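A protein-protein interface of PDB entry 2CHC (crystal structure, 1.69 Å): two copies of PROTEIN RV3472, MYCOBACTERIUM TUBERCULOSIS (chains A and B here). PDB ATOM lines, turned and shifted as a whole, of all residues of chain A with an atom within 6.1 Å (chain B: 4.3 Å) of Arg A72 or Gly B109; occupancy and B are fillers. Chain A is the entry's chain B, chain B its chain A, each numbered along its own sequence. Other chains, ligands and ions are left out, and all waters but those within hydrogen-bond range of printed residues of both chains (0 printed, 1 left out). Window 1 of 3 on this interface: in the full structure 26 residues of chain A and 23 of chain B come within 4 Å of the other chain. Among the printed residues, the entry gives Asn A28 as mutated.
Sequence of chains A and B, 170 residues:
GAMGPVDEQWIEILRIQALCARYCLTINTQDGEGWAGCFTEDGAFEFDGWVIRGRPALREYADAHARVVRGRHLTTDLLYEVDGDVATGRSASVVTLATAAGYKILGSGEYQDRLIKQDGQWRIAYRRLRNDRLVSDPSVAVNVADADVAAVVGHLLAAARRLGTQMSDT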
ATOM      1  N   CYS A  24      -8.631 -16.800   9.599  1.00  0.00           N
ATOM      2  CA  CYS A  24      -8.974 -15.481  10.118  1.00  0.00           C
ATOM      3  C   CYS A  24      -9.895 -14.772   9.113  1.00  0.00           C
ATOM      4  O   CYS A  24     -10.901 -14.140   9.474  1.00  0.00           O
ATOM      5  CB  CYS A  24      -7.728 -14.693  10.291  1.00  0.00           C
ATOM      6  SG  CYS A  24      -6.662 -15.315  11.559  1.00  0.00           S
ATOM      7  N   LEU A  25      -9.565 -14.846   7.829  1.00  0.00           N
ATOM      8  CA  LEU A  25     -10.317 -14.075   6.831  1.00  0.00           C
ATOM      9  C   LEU A  25     -11.753 -14.561   6.653  1.00  0.00           C
ATOM     10  O   LEU A  25     -12.649 -13.729   6.457  1.00  0.00           O
ATOM     11  CB  LEU A  25      -9.609 -14.091   5.463  1.00  0.00           C
ATOM     12  CG  LEU A  25      -8.327 -13.273   5.498  1.00  0.00           C
ATOM     13  CD1 LEU A  25      -7.519 -13.696   4.277  1.00  0.00           C
ATOM     14  CD2 LEU A  25      -8.504 -11.731   5.532  1.00  0.00           C
ATOM     15  N   ASN A  28     -13.804 -13.511   9.826  1.00  0.00           N
ATOM     16  CA  ASN A  28     -13.904 -12.059   9.909  1.00  0.00           C
ATOM     17  C   ASN A  28     -14.765 -11.512   8.811  1.00  0.00           C
ATOM     18  O   ASN A  28     -15.100 -10.347   8.831  1.00  0.00           O
ATOM     19  CB  ASN A  28     -12.525 -11.409   9.906  1.00  0.00           C
ATOM     20  CG  ASN A  28     -11.715 -11.642  11.158  1.00  0.00           C
ATOM     21  OD1 ASN A  28     -10.506 -11.489  11.137  1.00  0.00           O
ATOM     22  ND2 ASN A  28     -12.341 -12.017  12.197  1.00  0.00           N
ATOM     23  N   THR A  29     -15.132 -12.323   7.835  1.00  0.00           N
ATOM     24  CA  THR A  29     -16.117 -11.892   6.840  1.00  0.00           C
ATOM     25  C   THR A  29     -17.429 -12.687   6.947  1.00  0.00           C
ATOM     26  O   THR A  29     -18.250 -12.676   6.024  1.00  0.00           O
ATOM     27  CB  THR A  29     -15.509 -11.981   5.461  1.00  0.00           C
ATOM     28  OG1 THR A  29     -15.162 -13.310   5.138  1.00  0.00           O
ATOM     29  CG2 THR A  29     -14.243 -11.215   5.401  1.00  0.00           C
ATOM     30  N   ARG A  70     -17.761  -7.822  15.227  1.00  0.00           N
ATOM     31  CA  ARG A  70     -17.040  -7.315  14.062  1.00  0.00           C
ATOM     32  C   ARG A  70     -15.634  -6.937  14.608  1.00  0.00           C
ATOM     33  O   ARG A  70     -15.504  -6.204  15.609  1.00  0.00           O
ATOM     34  CB  ARG A  70     -17.716  -6.098  13.439  1.00  0.00           C
ATOM     35  CG  ARG A  70     -19.030  -6.384  12.678  1.00  0.00           C
ATOM     36  CD  ARG A  70     -18.895  -7.317  11.516  1.00  0.00           C
ATOM     37  NE  ARG A  70     -20.176  -7.606  10.860  1.00  0.00           N
ATOM     38  CZ  ARG A  70     -20.977  -8.621  11.175  1.00  0.00           C
ATOM     39  NH1 ARG A  70     -22.121  -8.807  10.498  1.00  0.00           N
ATOM     40  NH2 ARG A  70     -20.670  -9.428  12.172  1.00  0.00           N
ATOM     41  N   GLY A  71     -14.645  -7.401  13.918  1.00  0.00           N
ATOM     42  CA  GLY A  71     -13.258  -7.155  14.288  1.00  0.00           C
ATOM     43  C   GLY A  71     -12.381  -8.038  13.475  1.00  0.00           C
ATOM     44  O   GLY A  71     -12.842  -8.664  12.481  1.00  0.00           O
ATOM     45  N   ARG A  72     -11.114  -8.083  13.865  1.00  0.00           N
ATOM     46  CA  ARG A  72     -10.057  -8.755  13.117  1.00  0.00           C
ATOM     47  C   ARG A  72      -9.422  -9.777  13.995  1.00  0.00           C
ATOM     48  O   ARG A  72      -9.018  -9.424  15.090  1.00  0.00           O
ATOM     49  CB  ARG A  72      -8.872  -7.822  12.729  1.00  0.00           C
ATOM     50  CG  ARG A  72      -8.725  -7.223  11.462  1.00  0.00           C
ATOM     51  CD  ARG A  72      -9.168  -8.080  10.327  1.00  0.00           C
ATOM     52  NE  ARG A  72     -10.475  -7.694   9.886  1.00  0.00           N
ATOM     53  CZ  ARG A  72     -11.044  -8.162   8.791  1.00  0.00           C
ATOM     54  NH1 ARG A  72     -12.208  -7.768   8.444  1.00  0.00           N
ATOM     55  NH2 ARG A  72     -10.435  -9.090   8.034  1.00  0.00           N
ATOM     56  N   HIS A  73      -9.211 -10.992  13.484  1.00  0.00           N
ATOM     57  CA  HIS A  73      -8.335 -11.973  14.077  1.00  0.00           C
ATOM     58  C   HIS A  73      -6.992 -11.836  13.378  1.00  0.00           C
ATOM     59  O   HIS A  73      -6.961 -11.928  12.144  1.00  0.00           O
ATOM     60  CB  HIS A  73      -8.854 -13.374  13.780  1.00  0.00           C
ATOM     61  CG  HIS A  73     -10.040 -13.736  14.587  1.00  0.00           C
ATOM     62  ND1 HIS A  73     -11.300 -13.247  14.319  1.00  0.00           N
ATOM     63  CD2 HIS A  73     -10.149 -14.465  15.719  1.00  0.00           C
ATOM     64  CE1 HIS A  73     -12.134 -13.696  15.238  1.00  0.00           C
ATOM     65  NE2 HIS A  73     -11.475 -14.466  16.074  1.00  0.00           N
ATOM     66  N   LEU A  74      -5.956 -11.510  14.125  1.00  0.00           N
ATOM     67  CA  LEU A  74      -4.585 -11.492  13.644  1.00  0.00           C
ATOM     68  C   LEU A  74      -3.886 -12.746  14.086  1.00  0.00           C
ATOM     69  O   LEU A  74      -3.979 -13.123  15.285  1.00  0.00           O
ATOM     70  CB  LEU A  74      -3.869 -10.298  14.260  1.00  0.00           C
ATOM     71  CG  LEU A  74      -4.483  -8.961  14.109  1.00  0.00           C
ATOM     72  CD1 LEU A  74      -3.448  -7.924  14.695  1.00  0.00           C
ATOM     73  CD2 LEU A  74      -4.774  -8.603  12.666  1.00  0.00           C
ATOM     74  N   VAL A  94      -4.147 -12.248  18.258  1.00  0.00           N
ATOM     75  CA  VAL A  94      -4.687 -10.977  18.856  1.00  0.00           C
ATOM     76  C   VAL A  94      -5.927 -10.703  18.062  1.00  0.00           C
ATOM     77  O   VAL A  94      -5.952 -10.781  16.857  1.00  0.00           O
ATOM     78  CB  VAL A  94      -3.695  -9.811  18.844  1.00  0.00           C
ATOM     79  CG1 VAL A  94      -4.344  -8.513  19.347  1.00  0.00           C
ATOM     80  CG2 VAL A  94      -2.519 -10.154  19.716  1.00  0.00           C
ATOM     81  N   VAL A  95      -7.001 -10.406  18.773  1.00  0.00           N
ATOM     82  CA  VAL A  95      -8.340 -10.240  18.198  1.00  0.00           C
ATOM     83  C   VAL A  95      -8.887  -8.886  18.596  1.00  0.00           C
ATOM     84  O   VAL A  95      -8.968  -8.576  19.776  1.00  0.00           O
ATOM     85  CB  VAL A  95      -9.291 -11.368  18.635  1.00  0.00           C
ATOM     86  CG1 VAL A  95     -10.610 -11.169  17.921  1.00  0.00           C
ATOM     87  CG2 VAL A  95      -8.710 -12.737  18.354  1.00  0.00           C
ATOM     88  N   THR A  96      -9.198  -8.037  17.600  1.00  0.00           N
ATOM     89  CA  THR A  96      -9.778  -6.732  17.862  1.00  0.00           C
ATOM     90  C   THR A  96     -11.271  -6.792  17.739  1.00  0.00           C
ATOM     91  O   THR A  96     -11.872  -7.764  17.201  1.00  0.00           O
ATOM     92  CB  THR A  96      -9.320  -5.678  16.925  1.00  0.00           C
ATOM     93  OG1 THR A  96      -9.805  -6.014  15.600  1.00  0.00           O
ATOM     94  CG2 THR A  96      -7.846  -5.624  16.889  1.00  0.00           C
ATOM     95  N   LEU A  97     -11.925  -5.813  18.327  1.00  0.00           N
ATOM     96  CA  LEU A  97     -13.367  -5.776  18.359  1.00  0.00           C
ATOM     97  C   LEU A  97     -13.815  -4.321  18.227  1.00  0.00           C
ATOM     98  O   LEU A  97     -13.358  -3.445  18.949  1.00  0.00           O
ATOM     99  CB  LEU A  97     -13.857  -6.318  19.709  1.00  0.00           C
ATOM    100  CG  LEU A  97     -15.327  -6.309  20.053  1.00  0.00           C
ATOM    101  CD1 LEU A  97     -16.034  -7.326  19.148  1.00  0.00           C
ATOM    102  CD2 LEU A  97     -15.551  -6.607  21.507  1.00  0.00           C
ATOM    103  N   TYR A 103     -12.237   0.766  19.007  1.00  0.00           N
ATOM    104  CA  TYR A 103     -11.715  -0.565  18.844  1.00  0.00           C
ATOM    105  C   TYR A 103     -10.968  -0.987  20.131  1.00  0.00           C
ATOM    106  O   TYR A 103     -10.244  -0.171  20.766  1.00  0.00           O
ATOM    107  CB  TYR A 103     -10.754  -0.602  17.667  1.00  0.00           C
ATOM    108  CG  TYR A 103     -11.375  -0.362  16.327  1.00  0.00           C
ATOM    109  CD1 TYR A 103     -12.218  -1.290  15.740  1.00  0.00           C
ATOM    110  CD2 TYR A 103     -11.037   0.771  15.589  1.00  0.00           C
ATOM    111  CE1 TYR A 103     -12.784  -1.048  14.485  1.00  0.00           C
ATOM    112  CE2 TYR A 103     -11.631   1.018  14.320  1.00  0.00           C
ATOM    113  CZ  TYR A 103     -12.472   0.060  13.777  1.00  0.00           C
ATOM    114  OH  TYR A 103     -13.098   0.276  12.546  1.00  0.00           O
ATOM    115  N   SER B  91      -5.787  -9.172   3.032  1.00  0.00           N
ATOM    116  CA  SER B  91      -5.008  -9.267   4.227  1.00  0.00           C
ATOM    117  C   SER B  91      -5.667  -8.426   5.311  1.00  0.00           C
ATOM    118  O   SER B  91      -6.530  -7.571   5.064  1.00  0.00           O
ATOM    119  CB  SER B  91      -3.583  -8.801   3.982  1.00  0.00           C
ATOM    120  OG  SER B  91      -3.597  -7.515   3.439  1.00  0.00           O
ATOM    121  N   ALA B  92      -5.347  -8.780   6.547  1.00  0.00           N
ATOM    122  CA  ALA B  92      -5.808  -8.073   7.721  1.00  0.00           C
ATOM    123  C   ALA B  92      -4.985  -6.826   8.013  1.00  0.00           C
ATOM    124  O   ALA B  92      -3.783  -6.885   7.957  1.00  0.00           O
ATOM    125  CB  ALA B  92      -5.809  -9.001   8.950  1.00  0.00           C
ATOM    126  N   SER B  93      -5.660  -5.749   8.395  1.00  0.00           N
ATOM    127  CA  SER B  93      -5.062  -4.463   8.752  1.00  0.00           C
ATOM    128  C   SER B  93      -5.452  -4.130  10.179  1.00  0.00           C
ATOM    129  O   SER B  93      -6.659  -4.124  10.513  1.00  0.00           O
ATOM    130  CB  SER B  93      -5.623  -3.334   7.874  1.00  0.00           C
ATOM    131  OG  SER B  93      -5.102  -2.120   8.409  1.00  0.00           O
ATOM    132  N   VAL B  94      -4.471  -3.886  11.043  1.00  0.00           N
ATOM    133  CA  VAL B  94      -4.723  -3.279  12.362  1.00  0.00           C
ATOM    134  C   VAL B  94      -3.737  -2.147  12.502  1.00  0.00           C
ATOM    135  O   VAL B  94      -2.560  -2.284  12.133  1.00  0.00           O
ATOM    136  CB  VAL B  94      -4.641  -4.265  13.527  1.00  0.00           C
ATOM    137  CG1 VAL B  94      -4.726  -3.533  14.838  1.00  0.00           C
ATOM    138  CG2 VAL B  94      -5.796  -5.219  13.398  1.00  0.00           C
ATOM    139  N   SER B 108      -9.067  -1.108  12.274  1.00  0.00           N
ATOM    140  CA  SER B 108      -9.112  -2.548  12.103  1.00  0.00           C
ATOM    141  C   SER B 108      -9.955  -2.837  10.895  1.00  0.00           C
ATOM    142  O   SER B 108     -11.043  -2.267  10.776  1.00  0.00           O
ATOM    143  CB  SER B 108      -9.728  -3.062  13.385  1.00  0.00           C
ATOM    144  OG  SER B 108     -10.033  -4.363  13.398  1.00  0.00           O
ATOM    145  N   GLY B 109      -9.456  -3.641   9.971  1.00  0.00           N
ATOM    146  CA  GLY B 109     -10.174  -3.981   8.760  1.00  0.00           C
ATOM    147  C   GLY B 109      -9.380  -4.863   7.848  1.00  0.00           C
ATOM    148  O   GLY B 109      -8.517  -5.590   8.293  1.00  0.00           O
ATOM    149  N   GLU B 110      -9.795  -4.874   6.602  1.00  0.00           N
ATOM    150  CA  GLU B 110      -9.259  -5.758   5.590  1.00  0.00           C
ATOM    151  C   GLU B 110      -8.816  -4.971   4.394  1.00  0.00           C
ATOM    152  O   GLU B 110      -9.545  -4.104   3.915  1.00  0.00           O
ATOM    153  CB  GLU B 110     -10.374  -6.696   5.156  1.00  0.00           C
ATOM    154  CG  GLU B 110      -9.934  -7.741   4.216  1.00  0.00           C
ATOM    155  CD  GLU B 110     -11.092  -8.665   3.780  1.00  0.00           C
ATOM    156  OE1 GLU B 110     -11.982  -8.212   3.074  1.00  0.00           O
ATOM    157  OE2 GLU B 110     -11.122  -9.846   4.154  1.00  0.00           O
ATOM    158  N   ARG B 130     -11.331  -1.795   3.874  1.00  0.00           N
ATOM    159  CA  ARG B 130     -12.679  -1.838   4.476  1.00  0.00           C
ATOM    160  C   ARG B 130     -12.517  -1.963   5.970  1.00  0.00           C
ATOM    161  O   ARG B 130     -12.021  -2.983   6.411  1.00  0.00           O
ATOM    162  CB  ARG B 130     -13.361  -3.087   4.002  1.00  0.00           C
ATOM    163  N   ASN B 131     -12.909  -0.936   6.734  1.00  0.00           N
ATOM    164  CA  ASN B 131     -12.714  -0.945   8.185  1.00  0.00           C
ATOM    165  C   ASN B 131     -13.905  -1.654   8.845  1.00  0.00           C
ATOM    166  O   ASN B 131     -15.051  -1.654   8.327  1.00  0.00           O
ATOM    167  CB  ASN B 131     -12.404   0.488   8.735  1.00  0.00           C
ATOM    168  CG  ASN B 131     -10.898   0.683   9.225  1.00  0.00           C
ATOM    169  OD1 ASN B 131     -10.681   1.429  10.192  1.00  0.00           O
ATOM    170  ND2 ASN B 131      -9.936  -0.083   8.693  1.00  0.00           N
ATOM    171  N   ASP B 132     -13.631  -2.364   9.936  1.00  0.00           N
ATOM    172  CA  ASP B 132     -14.634  -3.093  10.642  1.00  0.00           C
ATOM    173  C   ASP B 132     -15.582  -2.133  11.344  1.00  0.00           C
ATOM    174  O   ASP B 132     -15.150  -1.132  11.911  1.00  0.00           O
ATOM    175  CB  ASP B 132     -13.977  -4.017  11.636  1.00  0.00           C
ATOM    176  CG  ASP B 132     -13.028  -5.026  10.967  1.00  0.00           C
ATOM    177  OD1 ASP B 132     -13.387  -5.591   9.935  1.00  0.00           O
ATOM    178  OD2 ASP B 132     -11.936  -5.277  11.486  1.00  0.00           O
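NH1 of Arg A72 is in salt-bridge range of OD1 of Asp B132 (2.9 Å). O of Gly B109 sits close to NE of Arg A72 (3.3 Å). The side-chain hydroxyl of Ser B108 lies within hydrogen-bond range of the side-chain hydroxyl of Thr A96, 2.8 Å away. OH of Tyr A103 sits at hydrogen-bond distance from O of Asp B132.
The side-chain amide nitrogen (ND2) of Asn A28 lies within hydrogen-bond range of the backbone carbonyl oxygen (O) of Gly A71. O of Ser B108 is in hydrogen-bond range of ND2 of Asn B131, 3.2 Å away. N of Arg B130 sits at hydrogen-bond distance from O of Glu B110 (2.9 Å). O of Arg A72 lies within hydrogen-bond range of N of Thr A96. O of Ser B108 sits at hydrogen-bond distance from N of Asp B132 (2.7 Å). The side-chain hydroxyl (OG1) of Thr A29 is in hydrogen-bond range of the backbone carbonyl oxygen (O) of Leu A25 (2.9 Å).
Among the printed residues, merely in contact across the chains: Leu A25 with Glu B110, Thr A29 with Glu B110, Gly A71 with Asp B132, Arg A72 with Ala B92, Arg A72 with Ser B93, Arg A72 with Ser B108, Arg A72 with Glu B110, Leu A74 with Ala B92, Leu A74 with Val B94, Tyr A103 with Ser B108 and Tyr A103 with Asn B131.
Arg A72 touches six residues of chain B. Gly B109 touches just one residue of chain A: Arg A72 (3.3 Å). Printed residues of chain A within 4 Å of Ala B92: Arg A72 (3.7 Å) and Leu A74 (3.9 Å). Of the printed residues of chain A, Asp B132 touches Gly A71, Arg A72 and Tyr A103. Printed residues of chain B within 4 Å of Thr A96: Ser B108. Of the printed residues of chain B, Thr A29 touches Glu B110. Of the printed residues of chain A, Val B94 touches Leu A74 (3.6 Å).
Hydrophobic or aromatic side chains of chain A that line the printed part of chain B: Leu A25, Leu A74 and Tyr A103. Of the 10 printed residues of chain B, 8 touch a printed residue of chain A. Hydrophobic or aromatic side chains of chain B that line the printed part of chain A: Ala B92 and Val B94.
1 position is printed for both chains. Of the 15 pairs that touch across the chains among the printed residues, none has its exchanged pair printed and touching as well.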
